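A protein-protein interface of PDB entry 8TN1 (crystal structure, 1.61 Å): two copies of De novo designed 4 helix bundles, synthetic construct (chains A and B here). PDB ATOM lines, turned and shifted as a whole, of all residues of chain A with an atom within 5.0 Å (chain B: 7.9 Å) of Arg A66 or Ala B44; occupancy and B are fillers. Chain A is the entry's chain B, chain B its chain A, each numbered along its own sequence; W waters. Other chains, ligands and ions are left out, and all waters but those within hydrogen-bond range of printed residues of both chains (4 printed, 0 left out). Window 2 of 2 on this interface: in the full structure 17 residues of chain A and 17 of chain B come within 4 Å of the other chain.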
ATOM      1  N   GLN A  59      36.082 -12.290 -16.437  1.00  0.00           N
ATOM      2  CA  GLN A  59      34.852 -12.949 -16.005  1.00  0.00           C
ATOM      3  C   GLN A  59      34.188 -12.194 -14.855  1.00  0.00           C
ATOM      4  O   GLN A  59      32.963 -12.022 -14.834  1.00  0.00           O
ATOM      5  CB  GLN A  59      35.173 -14.395 -15.634  1.00  0.00           C
ATOM      6  CG  GLN A  59      33.989 -15.198 -15.074  1.00  0.00           C
ATOM      7  CD  GLN A  59      32.886 -15.347 -16.073  1.00  0.00           C
ATOM      8  OE1 GLN A  59      33.129 -15.508 -17.255  1.00  0.00           O
ATOM      9  NE2 GLN A  59      31.651 -15.303 -15.597  1.00  0.00           N
ATOM     10  N   VAL A  62      32.513  -9.137 -16.362  1.00  0.00           N
ATOM     11  CA  VAL A  62      31.230  -9.501 -16.976  1.00  0.00           C
ATOM     12  C   VAL A  62      30.151  -9.681 -15.918  1.00  0.00           C
ATOM     13  O   VAL A  62      29.025  -9.196 -16.061  1.00  0.00           O
ATOM     14  CB  VAL A  62      31.413 -10.786 -17.801  1.00  0.00           C
ATOM     15  CG1 VAL A  62      30.041 -11.330 -18.236  1.00  0.00           C
ATOM     16  CG2 VAL A  62      32.315 -10.554 -19.006  1.00  0.00           C
ATOM     17  N   GLU A  63      30.472 -10.403 -14.846  1.00  0.00           N
ATOM     18  CA  GLU A  63      29.510 -10.622 -13.776  1.00  0.00           C
ATOM     19  C   GLU A  63      29.060  -9.307 -13.165  1.00  0.00           C
ATOM     20  O   GLU A  63      27.890  -9.146 -12.802  1.00  0.00           O
ATOM     21  CB  GLU A  63      30.126 -11.504 -12.701  1.00  0.00           C
ATOM     22  CG  GLU A  63      30.467 -12.875 -13.180  1.00  0.00           C
ATOM     23  CD  GLU A  63      31.140 -13.736 -12.112  1.00  0.00           C
ATOM     24  OE1 GLU A  63      31.098 -13.380 -10.910  1.00  0.00           O
ATOM     25  OE2 GLU A  63      31.652 -14.808 -12.489  1.00  0.00           O
ATOM     26  N   THR A  64      30.002  -8.366 -13.023  1.00  0.00           N
ATOM     27  CA  THR A  64      29.710  -7.070 -12.441  1.00  0.00           C
ATOM     28  C   THR A  64      28.720  -6.313 -13.315  1.00  0.00           C
ATOM     29  O   THR A  64      27.752  -5.724 -12.820  1.00  0.00           O
ATOM     30  CB  THR A  64      31.024  -6.291 -12.279  1.00  0.00           C
ATOM     31  OG1 THR A  64      31.888  -6.985 -11.358  1.00  0.00           O
ATOM     32  CG2 THR A  64      30.788  -4.889 -11.777  1.00  0.00           C
ATOM     33  N   VAL A  65      28.949  -6.310 -14.631  1.00  0.00           N
ATOM     34  CA  VAL A  65      27.981  -5.683 -15.536  1.00  0.00           C
ATOM     35  C   VAL A  65      26.625  -6.375 -15.403  1.00  0.00           C
ATOM     36  O   VAL A  65      25.591  -5.724 -15.274  1.00  0.00           O
ATOM     37  CB  VAL A  65      28.494  -5.684 -16.986  1.00  0.00           C
ATOM     38  CG1 VAL A  65      27.396  -5.278 -18.002  1.00  0.00           C
ATOM     39  CG2 VAL A  65      29.719  -4.728 -17.109  1.00  0.00           C
ATOM     40  N   ARG A  66      26.603  -7.707 -15.432  1.00  0.00           N
ATOM     41  CA  ARG A  66      25.311  -8.393 -15.338  1.00  0.00           C
ATOM     42  C   ARG A  66      24.547  -8.021 -14.073  1.00  0.00           C
ATOM     43  O   ARG A  66      23.327  -7.832 -14.115  1.00  0.00           O
ATOM     44  CB  ARG A  66      25.550  -9.884 -15.393  1.00  0.00           C
ATOM     45  CG  ARG A  66      25.884 -10.349 -16.756  1.00  0.00           C
ATOM     46  CD  ARG A  66      25.939 -11.859 -16.758  1.00  0.00           C
ATOM     47  NE  ARG A  66      26.625 -12.394 -17.926  1.00  0.00           N
ATOM     48  CZ  ARG A  66      27.401 -13.469 -17.906  1.00  0.00           C
ATOM     49  NH1 ARG A  66      27.618 -14.146 -16.787  1.00  0.00           N
ATOM     50  NH2 ARG A  66      27.938 -13.898 -19.043  1.00  0.00           N
ATOM     51  N   LEU A  67      25.247  -7.917 -12.943  1.00  0.00           N
ATOM     52  CA  LEU A  67      24.604  -7.577 -11.685  1.00  0.00           C
ATOM     53  C   LEU A  67      24.056  -6.151 -11.720  1.00  0.00           C
ATOM     54  O   LEU A  67      22.924  -5.902 -11.287  1.00  0.00           O
ATOM     55  CB  LEU A  67      25.594  -7.738 -10.553  1.00  0.00           C
ATOM     56  CG  LEU A  67      25.806  -9.175 -10.091  1.00  0.00           C
ATOM     57  CD1 LEU A  67      27.086  -9.244  -9.332  1.00  0.00           C
ATOM     58  CD2 LEU A  67      24.643  -9.630  -9.229  1.00  0.00           C
ATOM     59  N   LEU A  68      24.824  -5.211 -12.272  1.00  0.00           N
ATOM     60  CA  LEU A  68      24.350  -3.834 -12.313  1.00  0.00           C
ATOM     61  C   LEU A  68      23.210  -3.669 -13.305  1.00  0.00           C
ATOM     62  O   LEU A  68      22.310  -2.844 -13.079  1.00  0.00           O
ATOM     63  CB  LEU A  68      25.494  -2.873 -12.657  1.00  0.00           C
ATOM     64  CG  LEU A  68      26.345  -2.693 -11.415  1.00  0.00           C
ATOM     65  CD1 LEU A  68      27.750  -2.148 -11.737  1.00  0.00           C
ATOM     66  CD2 LEU A  68      25.643  -1.796 -10.416  1.00  0.00           C
ATOM     67  N   ALA A  69      23.240  -4.423 -14.401  1.00  0.00           N
ATOM     68  CA  ALA A  69      22.122  -4.394 -15.341  1.00  0.00           C
ATOM     69  C   ALA A  69      20.866  -4.897 -14.676  1.00  0.00           C
ATOM     70  O   ALA A  69      19.774  -4.379 -14.928  1.00  0.00           O
ATOM     71  CB  ALA A  69      22.434  -5.234 -16.566  1.00  0.00           C
ATOM     72  N   GLU A  70      21.007  -5.906 -13.821  1.00  0.00           N
ATOM     73  CA  GLU A  70      19.880  -6.393 -13.041  1.00  0.00           C
ATOM     74  C   GLU A  70      19.444  -5.347 -12.025  1.00  0.00           C
ATOM     75  O   GLU A  70      18.246  -5.128 -11.834  1.00  0.00           O
ATOM     76  CB  GLU A  70      20.272  -7.713 -12.380  1.00  0.00           C
ATOM     77  CG  GLU A  70      19.310  -8.210 -11.325  1.00  0.00           C
ATOM     78  CD  GLU A  70      19.642  -9.611 -10.837  1.00  0.00           C
ATOM     79  OE1 GLU A  70      20.848  -9.936 -10.724  1.00  0.00           O
ATOM     80  OE2 GLU A  70      18.690 -10.380 -10.566  1.00  0.00           O
ATOM     81  N   ALA B  31      24.342 -21.957 -26.410  1.00  0.00           N
ATOM     82  CA  ALA B  31      24.168 -20.505 -26.380  1.00  0.00           C
ATOM     83  C   ALA B  31      23.275 -20.045 -27.527  1.00  0.00           C
ATOM     84  O   ALA B  31      22.386 -19.212 -27.332  1.00  0.00           O
ATOM     85  CB  ALA B  31      25.524 -19.815 -26.481  1.00  0.00           C
ATOM     86  N   ALA B  34      19.673 -20.887 -26.661  1.00  0.00           N
ATOM     87  CA  ALA B  34      19.183 -20.005 -25.613  1.00  0.00           C
ATOM     88  C   ALA B  34      18.877 -18.617 -26.174  1.00  0.00           C
ATOM     89  O   ALA B  34      17.855 -18.000 -25.826  1.00  0.00           O
ATOM     90  CB  ALA B  34      20.212 -19.925 -24.485  1.00  0.00           C
ATOM     91  N   TYR B  35      19.750 -18.115 -27.046  1.00  0.00           N
ATOM     92  CA  TYR B  35      19.510 -16.809 -27.662  1.00  0.00           C
ATOM     93  C   TYR B  35      18.229 -16.844 -28.472  1.00  0.00           C
ATOM     94  O   TYR B  35      17.380 -15.963 -28.330  1.00  0.00           O
ATOM     95  CB  TYR B  35      20.680 -16.406 -28.536  1.00  0.00           C
ATOM     96  CG  TYR B  35      20.416 -15.255 -29.502  1.00  0.00           C
ATOM     97  CD1 TYR B  35      20.326 -13.951 -29.053  1.00  0.00           C
ATOM     98  CD2 TYR B  35      20.227 -15.505 -30.844  1.00  0.00           C
ATOM     99  CE1 TYR B  35      20.078 -12.933 -29.926  1.00  0.00           C
ATOM    100  CE2 TYR B  35      19.962 -14.484 -31.723  1.00  0.00           C
ATOM    101  CZ  TYR B  35      19.906 -13.214 -31.257  1.00  0.00           C
ATOM    102  OH  TYR B  35      19.651 -12.181 -32.126  1.00  0.00           O
ATOM    103  N   ARG B  39      16.110 -16.946 -23.698  1.00  0.00           N
ATOM    104  CA  ARG B  39      16.406 -17.260 -22.306  1.00  0.00           C
ATOM    105  C   ARG B  39      17.761 -16.645 -21.954  1.00  0.00           C
ATOM    106  O   ARG B  39      18.786 -17.294 -22.098  1.00  0.00           O
ATOM    107  CB  ARG B  39      16.426 -18.759 -22.122  1.00  0.00           C
ATOM    108  CG  ARG B  39      15.086 -19.462 -22.403  1.00  0.00           C
ATOM    109  CD  ARG B  39      15.278 -20.971 -22.235  1.00  0.00           C
ATOM    110  NE  ARG B  39      15.885 -21.551 -23.428  1.00  0.00           N
ATOM    111  CZ  ARG B  39      17.069 -22.161 -23.491  1.00  0.00           C
ATOM    112  NH1 ARG B  39      17.838 -22.324 -22.424  1.00  0.00           N
ATOM    113  NH2 ARG B  39      17.487 -22.637 -24.659  1.00  0.00           N
ATOM    114  N   GLU B  40      17.733 -15.390 -21.478  1.00  0.00           N
ATOM    115  CA  GLU B  40      18.955 -14.613 -21.251  1.00  0.00           C
ATOM    116  C   GLU B  40      19.827 -15.169 -20.143  1.00  0.00           C
ATOM    117  O   GLU B  40      21.059 -15.069 -20.219  1.00  0.00           O
ATOM    118  CB  GLU B  40      18.634 -13.166 -20.870  1.00  0.00           C
ATOM    119  CG  GLU B  40      17.814 -12.363 -21.812  1.00  0.00           C
ATOM    120  CD  GLU B  40      17.882 -10.870 -21.438  1.00  0.00           C
ATOM    121  OE1 GLU B  40      17.900 -10.546 -20.223  1.00  0.00           O
ATOM    122  OE2 GLU B  40      17.956 -10.021 -22.347  1.00  0.00           O
ATOM    123  N   GLU B  41      19.221 -15.650 -19.051  1.00  0.00           N
ATOM    124  CA  GLU B  41      20.013 -16.223 -17.962  1.00  0.00           C
ATOM    125  C   GLU B  41      20.703 -17.507 -18.400  1.00  0.00           C
ATOM    126  O   GLU B  41      21.874 -17.739 -18.069  1.00  0.00           O
ATOM    127  CB  GLU B  41      19.107 -16.463 -16.756  1.00  0.00           C
ATOM    128  CG  GLU B  41      18.592 -15.149 -16.153  1.00  0.00           C
ATOM    129  CD  GLU B  41      17.831 -15.329 -14.856  1.00  0.00           C
ATOM    130  OE1 GLU B  41      18.015 -16.372 -14.200  1.00  0.00           O
ATOM    131  OE2 GLU B  41      17.059 -14.415 -14.499  1.00  0.00           O
ATOM    132  N   ASP B  42      19.998 -18.363 -19.147  1.00  0.00           N
ATOM    133  CA  ASP B  42      20.633 -19.539 -19.734  1.00  0.00           C
ATOM    134  C   ASP B  42      21.772 -19.135 -20.659  1.00  0.00           C
ATOM    135  O   ASP B  42      22.855 -19.707 -20.631  1.00  0.00           O
ATOM    136  CB  ASP B  42      19.605 -20.365 -20.524  1.00  0.00           C
ATOM    137  CG  ASP B  42      18.521 -20.992 -19.645  1.00  0.00           C
ATOM    138  OD1 ASP B  42      18.426 -20.678 -18.444  1.00  0.00           O
ATOM    139  OD2 ASP B  42      17.744 -21.806 -20.198  1.00  0.00           O
ATOM    140  N   LEU B  43      21.520 -18.160 -21.519  1.00  0.00           N
ATOM    141  CA  LEU B  43      22.539 -17.681 -22.430  1.00  0.00           C
ATOM    142  C   LEU B  43      23.789 -17.265 -21.674  1.00  0.00           C
ATOM    143  O   LEU B  43      24.913 -17.567 -22.117  1.00  0.00           O
ATOM    144  CB  LEU B  43      22.000 -16.495 -23.238  1.00  0.00           C
ATOM    145  CG  LEU B  43      23.010 -15.902 -24.224  1.00  0.00           C
ATOM    146  CD1 LEU B  43      23.593 -16.905 -25.178  1.00  0.00           C
ATOM    147  CD2 LEU B  43      22.411 -14.688 -24.978  1.00  0.00           C
ATOM    148  N   ALA B  44      23.616 -16.562 -20.562  1.00  0.00           N
ATOM    149  CA  ALA B  44      24.763 -16.118 -19.761  1.00  0.00           C
ATOM    150  C   ALA B  44      25.608 -17.299 -19.294  1.00  0.00           C
ATOM    151  O   ALA B  44      26.840 -17.281 -19.411  1.00  0.00           O
ATOM    152  CB  ALA B  44      24.303 -15.300 -18.554  1.00  0.00           C
ATOM    153  N   THR B  45      24.950 -18.343 -18.801  1.00  0.00           N
ATOM    154  CA  THR B  45      25.667 -19.536 -18.353  1.00  0.00           C
ATOM    155  C   THR B  45      26.436 -20.175 -19.498  1.00  0.00           C
ATOM    156  O   THR B  45      27.596 -20.586 -19.328  1.00  0.00           O
ATOM    157  CB  THR B  45      24.662 -20.481 -17.713  1.00  0.00           C
ATOM    158  OG1 THR B  45      24.188 -19.850 -16.505  1.00  0.00           O
ATOM    159  CG2 THR B  45      25.265 -21.821 -17.421  1.00  0.00           C
ATOM    160  N   TYR B  46      25.822 -20.262 -20.677  1.00  0.00           N
ATOM    161  CA  TYR B  46      26.485 -20.946 -21.768  1.00  0.00           C
ATOM    162  C   TYR B  46      27.626 -20.126 -22.322  1.00  0.00           C
ATOM    163  O   TYR B  46      28.642 -20.678 -22.737  1.00  0.00           O
ATOM    164  CB  TYR B  46      25.501 -21.275 -22.869  1.00  0.00           C
ATOM    165  CG  TYR B  46      24.521 -22.356 -22.447  1.00  0.00           C
ATOM    166  CD1 TYR B  46      24.984 -23.530 -21.850  1.00  0.00           C
ATOM    167  CD2 TYR B  46      23.185 -22.199 -22.625  1.00  0.00           C
ATOM    168  CE1 TYR B  46      24.091 -24.527 -21.454  1.00  0.00           C
ATOM    169  CE2 TYR B  46      22.279 -23.220 -22.221  1.00  0.00           C
ATOM    170  CZ  TYR B  46      22.779 -24.353 -21.636  1.00  0.00           C
ATOM    171  OH  TYR B  46      21.949 -25.406 -21.269  1.00  0.00           O
ATOM    172  N   LEU B  47      27.450 -18.803 -22.364  1.00  0.00           N
ATOM    173  CA  LEU B  47      28.538 -17.930 -22.778  1.00  0.00           C
ATOM    174  C   LEU B  47      29.704 -18.025 -21.814  1.00  0.00           C
ATOM    175  O   LEU B  47      30.869 -17.979 -22.239  1.00  0.00           O
ATOM    176  CB  LEU B  47      28.047 -16.511 -22.882  1.00  0.00           C
ATOM    177  CG  LEU B  47      27.117 -16.286 -24.066  1.00  0.00           C
ATOM    178  CD1 LEU B  47      26.618 -14.810 -24.054  1.00  0.00           C
ATOM    179  CD2 LEU B  47      27.758 -16.651 -25.376  1.00  0.00           C
ATOM    180  N   ASP B  48      29.426 -18.101 -20.532  1.00  0.00           N
ATOM    181  CA  ASP B  48      30.548 -18.196 -19.593  1.00  0.00           C
ATOM    182  C   ASP B  48      31.292 -19.501 -19.772  1.00  0.00           C
ATOM    183  O   ASP B  48      32.523 -19.537 -19.657  1.00  0.00           O
ATOM    184  CB  ASP B  48      30.053 -18.080 -18.160  1.00  0.00           C
ATOM    185  CG  ASP B  48      29.639 -16.676 -17.802  1.00  0.00           C
ATOM    186  OD1 ASP B  48      29.897 -15.747 -18.595  1.00  0.00           O
ATOM    187  OD2 ASP B  48      29.107 -16.529 -16.699  1.00  0.00           O
ATOM    188  N   GLN B  49      30.563 -20.589 -20.029  1.00  0.00           N
ATOM    189  CA  GLN B  49      31.222 -21.850 -20.310  1.00  0.00           C
ATOM    190  C   GLN B  49      32.045 -21.722 -21.590  1.00  0.00           C
ATOM    191  O   GLN B  49      33.219 -22.099 -21.641  1.00  0.00           O
ATOM    192  CB  GLN B  49      30.182 -22.949 -20.410  1.00  0.00           C
ATOM    193  CG  GLN B  49      30.543 -24.326 -19.811  1.00  0.00           C
ATOM    194  CD  GLN B  49      31.064 -24.284 -18.371  1.00  0.00           C
ATOM    195  OE1 GLN B  49      30.897 -23.295 -17.647  1.00  0.00           O
ATOM    196  NE2 GLN B  49      31.618 -25.413 -17.922  1.00  0.00           N
ATOM    197  N   ALA B  50      31.452 -21.136 -22.624  1.00  0.00           N
ATOM    198  CA  ALA B  50      32.175 -20.997 -23.875  1.00  0.00           C
ATOM    199  C   ALA B  50      33.444 -20.190 -23.675  1.00  0.00           C
ATOM    200  O   ALA B  50      34.490 -20.535 -24.243  1.00  0.00           O
ATOM    201  CB  ALA B  50      31.277 -20.352 -24.931  1.00  0.00           C
ATOM    202  N   ALA B  51      33.378 -19.137 -22.862  1.00  0.00           N
ATOM    203  CA  ALA B  51      34.538 -18.275 -22.628  1.00  0.00           C
ATOM    204  C   ALA B  51      35.622 -19.055 -21.931  1.00  0.00           C
ATOM    205  O   ALA B  51      36.809 -18.907 -22.243  1.00  0.00           O
ATOM    206  CB  ALA B  51      34.128 -17.063 -21.824  1.00  0.00           C
ATOM    207  N   ALA B 104      31.008 -10.453 -27.947  1.00  0.00           N
ATOM    208  CA  ALA B 104      29.657 -10.980 -27.847  1.00  0.00           C
ATOM    209  C   ALA B 104      29.235 -11.076 -26.396  1.00  0.00           C
ATOM    210  O   ALA B 104      28.113 -10.701 -26.037  1.00  0.00           O
ATOM    211  CB  ALA B 104      29.598 -12.327 -28.528  1.00  0.00           C
ATOM    212  N   VAL B 105      30.145 -11.523 -25.529  1.00  0.00           N
ATOM    213  CA  VAL B 105      29.820 -11.677 -24.115  1.00  0.00           C
ATOM    214  C   VAL B 105      29.499 -10.329 -23.486  1.00  0.00           C
ATOM    215  O   VAL B 105      28.600 -10.223 -22.644  1.00  0.00           O
ATOM    216  CB  VAL B 105      30.972 -12.368 -23.350  1.00  0.00           C
ATOM    217  CG1 VAL B 105      30.786 -12.270 -21.863  1.00  0.00           C
ATOM    218  CG2 VAL B 105      31.092 -13.837 -23.690  1.00  0.00           C
ATOM    219  N   ALA B 106      30.251  -9.292 -23.854  1.00  0.00           N
ATOM    220  CA  ALA B 106      30.014  -7.972 -23.297  1.00  0.00           C
ATOM    221  C   ALA B 106      28.673  -7.438 -23.774  1.00  0.00           C
ATOM    222  O   ALA B 106      27.941  -6.805 -23.011  1.00  0.00           O
ATOM    223  CB  ALA B 106      31.129  -7.012 -23.707  1.00  0.00           C
ATOM    224  N   ALA B 108      26.001  -9.135 -24.750  1.00  0.00           N
ATOM    225  CA  ALA B 108      24.905  -9.827 -24.076  1.00  0.00           C
ATOM    226  C   ALA B 108      24.767  -9.323 -22.651  1.00  0.00           C
ATOM    227  O   ALA B 108      23.649  -9.189 -22.141  1.00  0.00           O
ATOM    228  CB  ALA B 108      25.141 -11.336 -24.133  1.00  0.00           C
ATOM    229  N   ALA B 109      25.891  -8.988 -22.006  1.00  0.00           N
ATOM    230  CA  ALA B 109      25.821  -8.509 -20.635  1.00  0.00           C
ATOM    231  C   ALA B 109      25.200  -7.121 -20.594  1.00  0.00           C
ATOM    232  O   ALA B 109      24.457  -6.809 -19.653  1.00  0.00           O
ATOM    233  CB  ALA B 109      27.216  -8.501 -20.005  1.00  0.00           C
ATOM    234  N   ASN B 110      25.524  -6.293 -21.600  1.00  0.00           N
ATOM    235  CA  ASN B 110      25.019  -4.927 -21.804  1.00  0.00           C
ATOM    236  C   ASN B 110      23.577  -4.912 -22.310  1.00  0.00           C
ATOM    237  O   ASN B 110      22.864  -3.915 -22.123  1.00  0.00           O
ATOM    238  CB  ASN B 110      25.915  -4.196 -22.851  1.00  0.00           C
ATOM    239  CG  ASN B 110      27.216  -3.613 -22.272  1.00  0.00           C
ATOM    240  OD1 ASN B 110      28.166  -4.330 -21.884  1.00  0.00           O
ATOM    241  ND2 ASN B 110      27.308  -2.279 -22.318  1.00  0.00           N
HETATM  242  O   HOH W   1      34.098 -17.988 -18.015  1.00  0.00           O
HETATM  243  O   HOH W   2      24.648 -11.873 -20.226  1.00  0.00           O
HETATM  244  O   HOH W   3      27.245 -12.080 -21.065  1.00  0.00           O
HETATM  245  O   HOH W   4      32.192 -14.744 -19.574  1.00  0.00           O
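Water W4 bridges OE1 of Gln A59 and OD1 of Asp B48.
Water W1 lies within hydrogen-bond range of O of Asp B48 (2.8 Å) and OE1 of Gln A59 (2.8 Å).
Water W3 lies within hydrogen-bond range of O of Val B105 (2.8 Å) and NH2 of Arg A66 (2.8 Å).
Water W2 bridges NE of Arg A66 (3.1 Å) and O of Ala B108 (3.4 Å).
OD2 of Asp B48 sits at hydrogen-bond distance from NE2 of Gln A59 (3.0 Å).
The side-chain carboxylate (OD1) of Asp B48 is in salt-bridge range of the guanidinium group (NH2) of Arg A66, at 2.7 Å.
No position is printed for both chains.
Of the 6 pairs that touch across the chains among the printed residues, none has its exchanged pair printed and touching as well.
Of the 10 printed residues of chain A, 4 touch a printed residue of chain B.
Hydrophobic or aromatic side chains of chain A within 4 Å of the printed part of chain B: Val A62 and Val A65.
Arg A66 touches just these residues of chain B: Ala B44, Asp B48 and Ala B109.
Of chain A, only Arg A66 comes within 4 Å of Ala B44.
Of the printed residues of chain B, Gln A59 touches Asp B48 (3.0 Å).
Printed residues of chain A within 4 Å of Val B105: Val A62.
Printed residues of chain B within 4 Å of Val A65: Ala B109.
Printed residues of chain A within 4 Å of Asp B48: Gln A59 and Arg A66.
Leu B43 touches none of the printed residues of chain A.
Ala A69 touches none of the printed residues of chain B.
The nearest residue of chain B that does not touch Arg A66 is Val B105 (4.3 Å).
The nearest printed residue of chain A that does not touch Ala B44 is Gln A59 (6.5 Å).
Among the printed residues, merely in contact across the chains: Val A62 with Val B105, Val A65 with Ala B109, Arg A66 with Ala B44 and Arg A66 with Ala B109.
NE2 of Gln A59 sits at hydrogen-bond distance from OE2 of Glu A63, at 3.1 Å.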
